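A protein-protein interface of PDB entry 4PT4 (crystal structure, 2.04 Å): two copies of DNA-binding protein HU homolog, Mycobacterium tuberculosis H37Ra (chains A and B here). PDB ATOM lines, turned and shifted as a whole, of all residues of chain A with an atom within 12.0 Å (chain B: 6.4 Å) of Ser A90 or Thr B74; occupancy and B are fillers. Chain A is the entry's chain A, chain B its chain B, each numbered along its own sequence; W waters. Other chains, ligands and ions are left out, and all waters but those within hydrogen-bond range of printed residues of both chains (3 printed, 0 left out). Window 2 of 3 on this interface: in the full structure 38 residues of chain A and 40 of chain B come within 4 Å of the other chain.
Water W2 lies within hydrogen-bond range of the guanidinium group of Arg B54 (2.6 Å), the backbone NH of Ser B75 (2.8 Å) and the backbone carbonyl oxygen of Ser A90 (3.3 Å).
Water W1 lies within hydrogen-bond range of the backbone carbonyl oxygen (O) of Val A88 (2.7 Å), the backbone carbonyl oxygen (O) of Gln A93 (2.7 Å) and a ring nitrogen (NE2) of His B37 (3.0 Å).
Water W3 lies within hydrogen-bond range of O of Ser B75 (2.7 Å) and O of Lys A86 (2.8 Å).
Pro B77 touches Pro A81.
Pro B77 touches Phe A85 (CB to CE1, 3.6 Å).
His B37 touches Val A89 (CD2 to CA, 3.97 Å).
Ser B75 touches Val A89 (O to CG1, 3.5 Å).
CG1 of Val A89 touches C of Val B76, at 3.9 Å.
Val A89 touches Pro B77.
Ser A90 touches Thr B74.
Ser A90 touches Ser B75 (CA to O, 3.6 Å).
Leu A95 touches His B37.
A ring nitrogen (NE2) of His B37 sits close to the backbone carbonyl oxygen of Val A88.
No position is printed for both chains.
Of the 10 pairs that touch across the chains among the printed residues, none has its exchanged pair printed and touching as well.
Printed residues of chain B within 4 Å of Pro A81: Pro B77.
Printed residues of chain B within 4 Å of Val A88: His B37 (3.2 Å).
Of the printed residues of chain B, Val A89 touches His B37, Ser B75, Val B76 and Pro B77.
Of chain B, only Thr B74 (3.5 Å) and Ser B75 (3.6 Å) come within 4 Å of Ser A90.
Gly A91 touches none of the printed residues of chain B.
Arg B54 touches none of the printed residues of chain A.
No residue of chain A comes within 4 Å of Arg B55.
No residue of chain A comes within 4 Å of Pro B73.
Thr B74 touches just one residue of chain A: Ser A90 (3.5 Å).
Ser B75 touches two residues of chain A.
Val B76 touches just one residue of chain A: Val A89.
Of the 13 printed residues of chain B, 5 touch a printed residue of chain A.
Along chain B the printed residues that touch a printed residue of chain A span positions 37 to 77.
Printed residues of chain A that touch a printed residue of chain B: Pro A81, Phe A85, Val A88, Val A89, Ser A90 and Leu A95.
The side-chain hydroxyl (OG) of Ser A90 lies within hydrogen-bond range of the backbone carbonyl oxygen (O) of Ala A87 (3.0 Å).
The backbone NH of Arg B55 lies within hydrogen-bond range of the backbone carbonyl oxygen of Thr B74, at 2.8 Å.
The backbone carbonyl oxygen (O) of Arg B53 is in hydrogen-bond range of the backbone NH (N) of Val B76 (2.6 Å).
OG of Ser A90 lies within hydrogen-bond range of O of Lys A86.
The backbone carbonyl oxygen (O) of Gly A46 lies within hydrogen-bond range of the backbone NH (N) of Phe A85 (3.2 Å).
The side-chain hydroxyl (OG) of Ser B75 lies within hydrogen-bond range of the guanidinium group (NH2) of Arg B54, 2.8 Å away.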
ATOM      1  N   GLY A  46       5.590  23.795 -21.676  1.00  0.00           N
ATOM      2  CA  GLY A  46       4.885  24.387 -20.560  1.00  0.00           C
ATOM      3  C   GLY A  46       5.134  23.616 -19.284  1.00  0.00           C
ATOM      4  O   GLY A  46       5.243  24.218 -18.215  1.00  0.00           O
ATOM      5  N   PHE A  47       5.247  22.290 -19.408  1.00  0.00           N
ATOM      6  CA  PHE A  47       5.394  21.375 -18.263  1.00  0.00           C
ATOM      7  C   PHE A  47       6.868  21.262 -17.922  1.00  0.00           C
ATOM      8  O   PHE A  47       7.274  21.573 -16.799  1.00  0.00           O
ATOM      9  CB  PHE A  47       4.799  20.027 -18.652  1.00  0.00           C
ATOM     10  CG  PHE A  47       4.780  18.997 -17.561  1.00  0.00           C
ATOM     11  CD1 PHE A  47       4.170  19.244 -16.337  1.00  0.00           C
ATOM     12  CD2 PHE A  47       5.308  17.736 -17.796  1.00  0.00           C
ATOM     13  CE1 PHE A  47       4.125  18.268 -15.368  1.00  0.00           C
ATOM     14  CE2 PHE A  47       5.229  16.752 -16.848  1.00  0.00           C
ATOM     15  CZ  PHE A  47       4.662  17.026 -15.624  1.00  0.00           C
ATOM     16  N   PRO A  81      11.832  21.533 -14.978  1.00  0.00           N
ATOM     17  CA  PRO A  81      10.493  22.147 -15.034  1.00  0.00           C
ATOM     18  C   PRO A  81      10.470  23.365 -15.914  1.00  0.00           C
ATOM     19  O   PRO A  81      11.329  24.196 -15.817  1.00  0.00           O
ATOM     20  CB  PRO A  81      10.234  22.535 -13.582  1.00  0.00           C
ATOM     21  CG  PRO A  81      10.975  21.525 -12.812  1.00  0.00           C
ATOM     22  CD  PRO A  81      12.266  21.339 -13.591  1.00  0.00           C
ATOM     23  N   GLY A  82       9.493  23.453 -16.791  1.00  0.00           N
ATOM     24  CA  GLY A  82       9.346  24.586 -17.695  1.00  0.00           C
ATOM     25  C   GLY A  82       8.801  25.799 -16.947  1.00  0.00           C
ATOM     26  O   GLY A  82       8.376  25.714 -15.778  1.00  0.00           O
ATOM     27  N   ALA A  83       8.877  26.935 -17.617  1.00  0.00           N
ATOM     28  CA  ALA A  83       8.554  28.235 -17.045  1.00  0.00           C
ATOM     29  C   ALA A  83       7.158  28.305 -16.460  1.00  0.00           C
ATOM     30  O   ALA A  83       6.970  28.812 -15.345  1.00  0.00           O
ATOM     31  CB  ALA A  83       8.727  29.304 -18.105  1.00  0.00           C
ATOM     32  N   GLN A  84       6.185  27.744 -17.161  1.00  0.00           N
ATOM     33  CA  GLN A  84       4.802  27.788 -16.684  1.00  0.00           C
ATOM     34  C   GLN A  84       4.509  26.889 -15.463  1.00  0.00           C
ATOM     35  O   GLN A  84       3.702  27.245 -14.588  1.00  0.00           O
ATOM     36  CB  GLN A  84       3.851  27.497 -17.852  1.00  0.00           C
ATOM     37  CG  GLN A  84       3.836  28.655 -18.849  1.00  0.00           C
ATOM     38  CD  GLN A  84       3.507  28.248 -20.278  1.00  0.00           C
ATOM     39  OE1 GLN A  84       2.705  27.343 -20.511  1.00  0.00           O
ATOM     40  NE2 GLN A  84       4.116  28.944 -21.248  1.00  0.00           N
ATOM     41  N   PHE A  85       5.152  25.737 -15.393  1.00  0.00           N
ATOM     42  CA  PHE A  85       5.079  24.908 -14.197  1.00  0.00           C
ATOM     43  C   PHE A  85       5.635  25.682 -12.992  1.00  0.00           C
ATOM     44  O   PHE A  85       4.993  25.746 -11.937  1.00  0.00           O
ATOM     45  CB  PHE A  85       5.852  23.595 -14.401  1.00  0.00           C
ATOM     46  CG  PHE A  85       5.477  22.468 -13.450  1.00  0.00           C
ATOM     47  CD1 PHE A  85       4.692  22.668 -12.333  1.00  0.00           C
ATOM     48  CD2 PHE A  85       5.988  21.202 -13.664  1.00  0.00           C
ATOM     49  CE1 PHE A  85       4.394  21.614 -11.476  1.00  0.00           C
ATOM     50  CE2 PHE A  85       5.707  20.150 -12.810  1.00  0.00           C
ATOM     51  CZ  PHE A  85       4.903  20.350 -11.726  1.00  0.00           C
ATOM     52  N   LYS A  86       6.826  26.254 -13.156  1.00  0.00           N
ATOM     53  CA  LYS A  86       7.436  27.074 -12.104  1.00  0.00           C
ATOM     54  C   LYS A  86       6.585  28.282 -11.709  1.00  0.00           C
ATOM     55  O   LYS A  86       6.504  28.639 -10.535  1.00  0.00           O
ATOM     56  CB  LYS A  86       8.798  27.574 -12.558  1.00  0.00           C
ATOM     57  CG  LYS A  86       9.908  26.569 -12.384  1.00  0.00           C
ATOM     58  CD  LYS A  86      10.763  26.395 -13.630  1.00  0.00           C
ATOM     59  CE  LYS A  86      11.741  27.515 -13.873  1.00  0.00           C
ATOM     60  NZ  LYS A  86      12.604  27.765 -12.683  1.00  0.00           N
ATOM     61  N   ALA A  87       6.004  28.933 -12.711  1.00  0.00           N
ATOM     62  CA  ALA A  87       5.313  30.197 -12.503  1.00  0.00           C
ATOM     63  C   ALA A  87       4.113  29.923 -11.640  1.00  0.00           C
ATOM     64  O   ALA A  87       3.865  30.634 -10.658  1.00  0.00           O
ATOM     65  CB  ALA A  87       4.922  30.848 -13.835  1.00  0.00           C
ATOM     66  N   VAL A  88       3.407  28.851 -11.981  1.00  0.00           N
ATOM     67  CA  VAL A  88       2.240  28.416 -11.235  1.00  0.00           C
ATOM     68  C   VAL A  88       2.559  28.032  -9.789  1.00  0.00           C
ATOM     69  O   VAL A  88       1.932  28.522  -8.869  1.00  0.00           O
ATOM     70  CB  VAL A  88       1.523  27.250 -11.968  1.00  0.00           C
ATOM     71  CG1 VAL A  88       0.529  26.541 -11.056  1.00  0.00           C
ATOM     72  CG2 VAL A  88       0.810  27.788 -13.201  1.00  0.00           C
ATOM     73  N   VAL A  89       3.520  27.146  -9.594  1.00  0.00           N
ATOM     74  CA  VAL A  89       3.900  26.716  -8.243  1.00  0.00           C
ATOM     75  C   VAL A  89       4.446  27.849  -7.369  1.00  0.00           C
ATOM     76  O   VAL A  89       4.198  27.870  -6.170  1.00  0.00           O
ATOM     77  CB  VAL A  89       4.937  25.564  -8.308  1.00  0.00           C
ATOM     78  CG1 VAL A  89       5.485  25.205  -6.944  1.00  0.00           C
ATOM     79  CG2 VAL A  89       4.293  24.359  -8.924  1.00  0.00           C
ATOM     80  N   SER A  90       5.214  28.774  -7.952  1.00  0.00           N
ATOM     81  CA  SER A  90       5.760  29.900  -7.189  1.00  0.00           C
ATOM     82  C   SER A  90       4.715  30.981  -6.859  1.00  0.00           C
ATOM     83  O   SER A  90       5.004  31.914  -6.087  1.00  0.00           O
ATOM     84  CB  SER A  90       6.903  30.560  -7.948  1.00  0.00           C
ATOM     85  OG  SER A  90       6.430  31.121  -9.166  1.00  0.00           O
ATOM     86  N   GLY A  91       3.531  30.887  -7.458  1.00  0.00           N
ATOM     87  CA  GLY A  91       2.464  31.886  -7.242  1.00  0.00           C
ATOM     88  C   GLY A  91       2.466  33.067  -8.209  1.00  0.00           C
ATOM     89  O   GLY A  91       1.664  33.995  -8.070  1.00  0.00           O
ATOM     90  N   ALA A  92       3.363  33.052  -9.193  1.00  0.00           N
ATOM     91  CA  ALA A  92       3.474  34.157 -10.142  1.00  0.00           C
ATOM     92  C   ALA A  92       2.455  34.082 -11.280  1.00  0.00           C
ATOM     93  O   ALA A  92       2.253  35.069 -11.996  1.00  0.00           O
ATOM     94  CB  ALA A  92       4.875  34.195 -10.721  1.00  0.00           C
ATOM     95  N   GLN A  93       1.864  32.908 -11.482  1.00  0.00           N
ATOM     96  CA  GLN A  93       0.767  32.736 -12.440  1.00  0.00           C
ATOM     97  C   GLN A  93      -0.316  31.841 -11.864  1.00  0.00           C
ATOM     98  O   GLN A  93      -0.019  30.793 -11.288  1.00  0.00           O
ATOM     99  CB  GLN A  93       1.249  32.115 -13.746  1.00  0.00           C
ATOM    100  N   ARG A  94      -1.569  32.245 -12.069  1.00  0.00           N
ATOM    101  CA  ARG A  94      -2.712  31.478 -11.639  1.00  0.00           C
ATOM    102  C   ARG A  94      -2.907  30.279 -12.554  1.00  0.00           C
ATOM    103  O   ARG A  94      -2.676  30.357 -13.735  1.00  0.00           O
ATOM    104  CB  ARG A  94      -3.982  32.353 -11.632  1.00  0.00           C
ATOM    105  N   LEU A  95      -3.329  29.166 -11.979  1.00  0.00           N
ATOM    106  CA  LEU A  95      -3.756  28.002 -12.736  1.00  0.00           C
ATOM    107  C   LEU A  95      -4.864  28.381 -13.725  1.00  0.00           C
ATOM    108  O   LEU A  95      -5.633  29.313 -13.458  1.00  0.00           O
ATOM    109  CB  LEU A  95      -4.307  26.942 -11.775  1.00  0.00           C
ATOM    110  CG  LEU A  95      -3.294  26.245 -10.887  1.00  0.00           C
ATOM    111  CD1 LEU A  95      -3.935  25.627  -9.647  1.00  0.00           C
ATOM    112  CD2 LEU A  95      -2.581  25.209 -11.718  1.00  0.00           C
ATOM    113  N   HIS B  37       0.924  21.836  -7.183  1.00  0.00           N
ATOM    114  CA  HIS B  37       0.588  23.190  -6.807  1.00  0.00           C
ATOM    115  C   HIS B  37       0.011  23.259  -5.439  1.00  0.00           C
ATOM    116  O   HIS B  37       0.374  24.104  -4.716  1.00  0.00           O
ATOM    117  CB  HIS B  37      -0.343  23.858  -7.792  1.00  0.00           C
ATOM    118  CG  HIS B  37      -0.685  25.251  -7.422  1.00  0.00           C
ATOM    119  ND1 HIS B  37      -1.866  25.580  -6.818  1.00  0.00           N
ATOM    120  CD2 HIS B  37      -0.004  26.403  -7.566  1.00  0.00           C
ATOM    121  CE1 HIS B  37      -1.904  26.877  -6.611  1.00  0.00           C
ATOM    122  NE2 HIS B  37      -0.783  27.399  -7.050  1.00  0.00           N
ATOM    123  N   ARG B  53       8.882  21.710  -3.713  1.00  0.00           N
ATOM    124  CA  ARG B  53       9.833  21.970  -2.638  1.00  0.00           C
ATOM    125  C   ARG B  53       9.924  23.447  -2.363  1.00  0.00           C
ATOM    126  O   ARG B  53       9.592  24.241  -3.205  1.00  0.00           O
ATOM    127  CB  ARG B  53      11.202  21.473  -3.028  1.00  0.00           C
ATOM    128  CG  ARG B  53      11.206  19.989  -3.327  1.00  0.00           C
ATOM    129  CD  ARG B  53      12.523  19.612  -3.909  1.00  0.00           C
ATOM    130  NE  ARG B  53      12.649  18.205  -4.235  1.00  0.00           N
ATOM    131  CZ  ARG B  53      13.626  17.730  -5.019  1.00  0.00           C
ATOM    132  NH1 ARG B  53      14.522  18.555  -5.530  1.00  0.00           N
ATOM    133  NH2 ARG B  53      13.707  16.444  -5.311  1.00  0.00           N
ATOM    134  N   ARG B  54      10.398  23.805  -1.186  1.00  0.00           N
ATOM    135  CA  ARG B  54      10.548  25.194  -0.810  1.00  0.00           C
ATOM    136  C   ARG B  54      12.027  25.496  -0.836  1.00  0.00           C
ATOM    137  O   ARG B  54      12.770  24.902  -0.078  1.00  0.00           O
ATOM    138  CB  ARG B  54       9.975  25.407   0.586  1.00  0.00           C
ATOM    139  CG  ARG B  54       9.828  26.872   1.013  1.00  0.00           C
ATOM    140  CD  ARG B  54       8.838  27.658   0.138  1.00  0.00           C
ATOM    141  NE  ARG B  54       8.466  28.944   0.754  1.00  0.00           N
ATOM    142  CZ  ARG B  54       7.765  29.919   0.165  1.00  0.00           C
ATOM    143  NH1 ARG B  54       7.496  31.016   0.853  1.00  0.00           N
ATOM    144  NH2 ARG B  54       7.337  29.820  -1.095  1.00  0.00           N
ATOM    145  N   ARG B  55      12.469  26.347  -1.758  1.00  0.00           N
ATOM    146  CA  ARG B  55      13.815  26.901  -1.711  1.00  0.00           C
ATOM    147  C   ARG B  55      13.821  28.101  -0.756  1.00  0.00           C
ATOM    148  O   ARG B  55      13.117  29.105  -0.956  1.00  0.00           O
ATOM    149  CB  ARG B  55      14.307  27.339  -3.080  1.00  0.00           C
ATOM    150  CG  ARG B  55      14.922  26.237  -3.930  1.00  0.00           C
ATOM    151  CD  ARG B  55      15.905  26.797  -4.936  1.00  0.00           C
ATOM    152  NE  ARG B  55      15.336  27.952  -5.617  1.00  0.00           N
ATOM    153  CZ  ARG B  55      15.044  28.012  -6.917  1.00  0.00           C
ATOM    154  NH1 ARG B  55      14.505  29.120  -7.416  1.00  0.00           N
ATOM    155  NH2 ARG B  55      15.277  26.977  -7.723  1.00  0.00           N
ATOM    156  N   ALA B  56      14.630  28.006   0.286  1.00  0.00           N
ATOM    157  CA  ALA B  56      14.670  29.065   1.262  1.00  0.00           C
ATOM    158  C   ALA B  56      16.076  29.577   1.376  1.00  0.00           C
ATOM    159  O   ALA B  56      17.021  28.772   1.451  1.00  0.00           O
ATOM    160  CB  ALA B  56      14.203  28.530   2.595  1.00  0.00           C
ATOM    161  N   ARG B  58      18.317  31.373  -0.442  1.00  0.00           N
ATOM    162  CA  ARG B  58      19.350  31.080  -1.422  1.00  0.00           C
ATOM    163  C   ARG B  58      20.064  32.385  -1.767  1.00  0.00           C
ATOM    164  O   ARG B  58      19.424  33.425  -1.917  1.00  0.00           O
ATOM    165  CB  ARG B  58      18.716  30.488  -2.677  1.00  0.00           C
ATOM    166  CG  ARG B  58      19.639  30.421  -3.875  1.00  0.00           C
ATOM    167  CD  ARG B  58      19.115  29.535  -4.995  1.00  0.00           C
ATOM    168  NE  ARG B  58      18.002  30.135  -5.750  1.00  0.00           N
ATOM    169  CZ  ARG B  58      18.115  30.999  -6.765  1.00  0.00           C
ATOM    170  NH1 ARG B  58      17.019  31.437  -7.383  1.00  0.00           N
ATOM    171  NH2 ARG B  58      19.297  31.436  -7.175  1.00  0.00           N
ATOM    172  N   VAL B  71      17.989  35.740  -2.294  1.00  0.00           N
ATOM    173  CA  VAL B  71      16.766  35.584  -3.059  1.00  0.00           C
ATOM    174  C   VAL B  71      15.613  35.223  -2.105  1.00  0.00           C
ATOM    175  O   VAL B  71      15.747  34.332  -1.278  1.00  0.00           O
ATOM    176  CB  VAL B  71      16.933  34.422  -4.048  1.00  0.00           C
ATOM    177  CG1 VAL B  71      15.678  34.247  -4.874  1.00  0.00           C
ATOM    178  CG2 VAL B  71      18.153  34.631  -4.947  1.00  0.00           C
ATOM    179  N   LYS B  72      14.462  35.877  -2.205  1.00  0.00           N
ATOM    180  CA  LYS B  72      13.393  35.509  -1.291  1.00  0.00           C
ATOM    181  C   LYS B  72      12.942  34.072  -1.551  1.00  0.00           C
ATOM    182  O   LYS B  72      12.995  33.587  -2.686  1.00  0.00           O
ATOM    183  CB  LYS B  72      12.211  36.484  -1.357  1.00  0.00           C
ATOM    184  CG  LYS B  72      11.244  36.269  -2.498  1.00  0.00           C
ATOM    185  CD  LYS B  72      10.418  37.520  -2.765  1.00  0.00           C
ATOM    186  CE  LYS B  72       9.432  37.781  -1.648  1.00  0.00           C
ATOM    187  NZ  LYS B  72       8.167  37.054  -1.914  1.00  0.00           N
ATOM    188  N   PRO B  73      12.499  33.390  -0.496  1.00  0.00           N
ATOM    189  CA  PRO B  73      12.055  32.005  -0.648  1.00  0.00           C
ATOM    190  C   PRO B  73      10.977  31.792  -1.727  1.00  0.00           C
ATOM    191  O   PRO B  73      10.174  32.686  -1.999  1.00  0.00           O
ATOM    192  CB  PRO B  73      11.546  31.660   0.760  1.00  0.00           C
ATOM    193  CG  PRO B  73      12.393  32.520   1.663  1.00  0.00           C
ATOM    194  CD  PRO B  73      12.464  33.818   0.922  1.00  0.00           C
ATOM    195  N   THR B  74      11.003  30.617  -2.350  1.00  0.00           N
ATOM    196  CA  THR B  74      10.072  30.281  -3.396  1.00  0.00           C
ATOM    197  C   THR B  74       9.743  28.798  -3.310  1.00  0.00           C
ATOM    198  O   THR B  74      10.556  27.999  -2.875  1.00  0.00           O
ATOM    199  CB  THR B  74      10.648  30.636  -4.785  1.00  0.00           C
ATOM    200  OG1 THR B  74       9.653  30.435  -5.798  1.00  0.00           O
ATOM    201  CG2 THR B  74      11.819  29.766  -5.127  1.00  0.00           C
ATOM    202  N   SER B  75       8.534  28.431  -3.705  1.00  0.00           N
ATOM    203  CA  SER B  75       8.185  27.040  -3.801  1.00  0.00           C
ATOM    204  C   SER B  75       8.462  26.605  -5.233  1.00  0.00           C
ATOM    205  O   SER B  75       8.123  27.328  -6.173  1.00  0.00           O
ATOM    206  CB  SER B  75       6.723  26.863  -3.458  1.00  0.00           C
ATOM    207  OG  SER B  75       6.481  27.438  -2.199  1.00  0.00           O
ATOM    208  N   VAL B  76       9.089  25.450  -5.411  1.00  0.00           N
ATOM    209  CA  VAL B  76       9.452  24.978  -6.753  1.00  0.00           C
ATOM    210  C   VAL B  76       9.021  23.526  -7.045  1.00  0.00           C
ATOM    211  O   VAL B  76       8.997  22.666  -6.143  1.00  0.00           O
ATOM    212  CB  VAL B  76      10.973  25.116  -7.024  1.00  0.00           C
ATOM    213  CG1 VAL B  76      11.421  26.569  -6.911  1.00  0.00           C
ATOM    214  CG2 VAL B  76      11.801  24.249  -6.080  1.00  0.00           C
ATOM    215  N   PRO B  77       8.684  23.250  -8.304  1.00  0.00           N
ATOM    216  CA  PRO B  77       8.375  21.895  -8.690  1.00  0.00           C
ATOM    217  C   PRO B  77       9.647  21.105  -8.883  1.00  0.00           C
ATOM    218  O   PRO B  77      10.672  21.674  -9.239  1.00  0.00           O
ATOM    219  CB  PRO B  77       7.662  22.064 -10.032  1.00  0.00           C
ATOM    220  CG  PRO B  77       8.198  23.309 -10.581  1.00  0.00           C
ATOM    221  CD  PRO B  77       8.583  24.180  -9.436  1.00  0.00           C
HETATM  222  O   HOH W   1      -0.350  29.870  -8.743  1.00  0.00           O
HETATM  223  O   HOH W   2       6.561  30.443  -3.517  1.00  0.00           O
HETATM  224  O   HOH W   3       8.533  27.543  -8.871  1.00  0.00           O
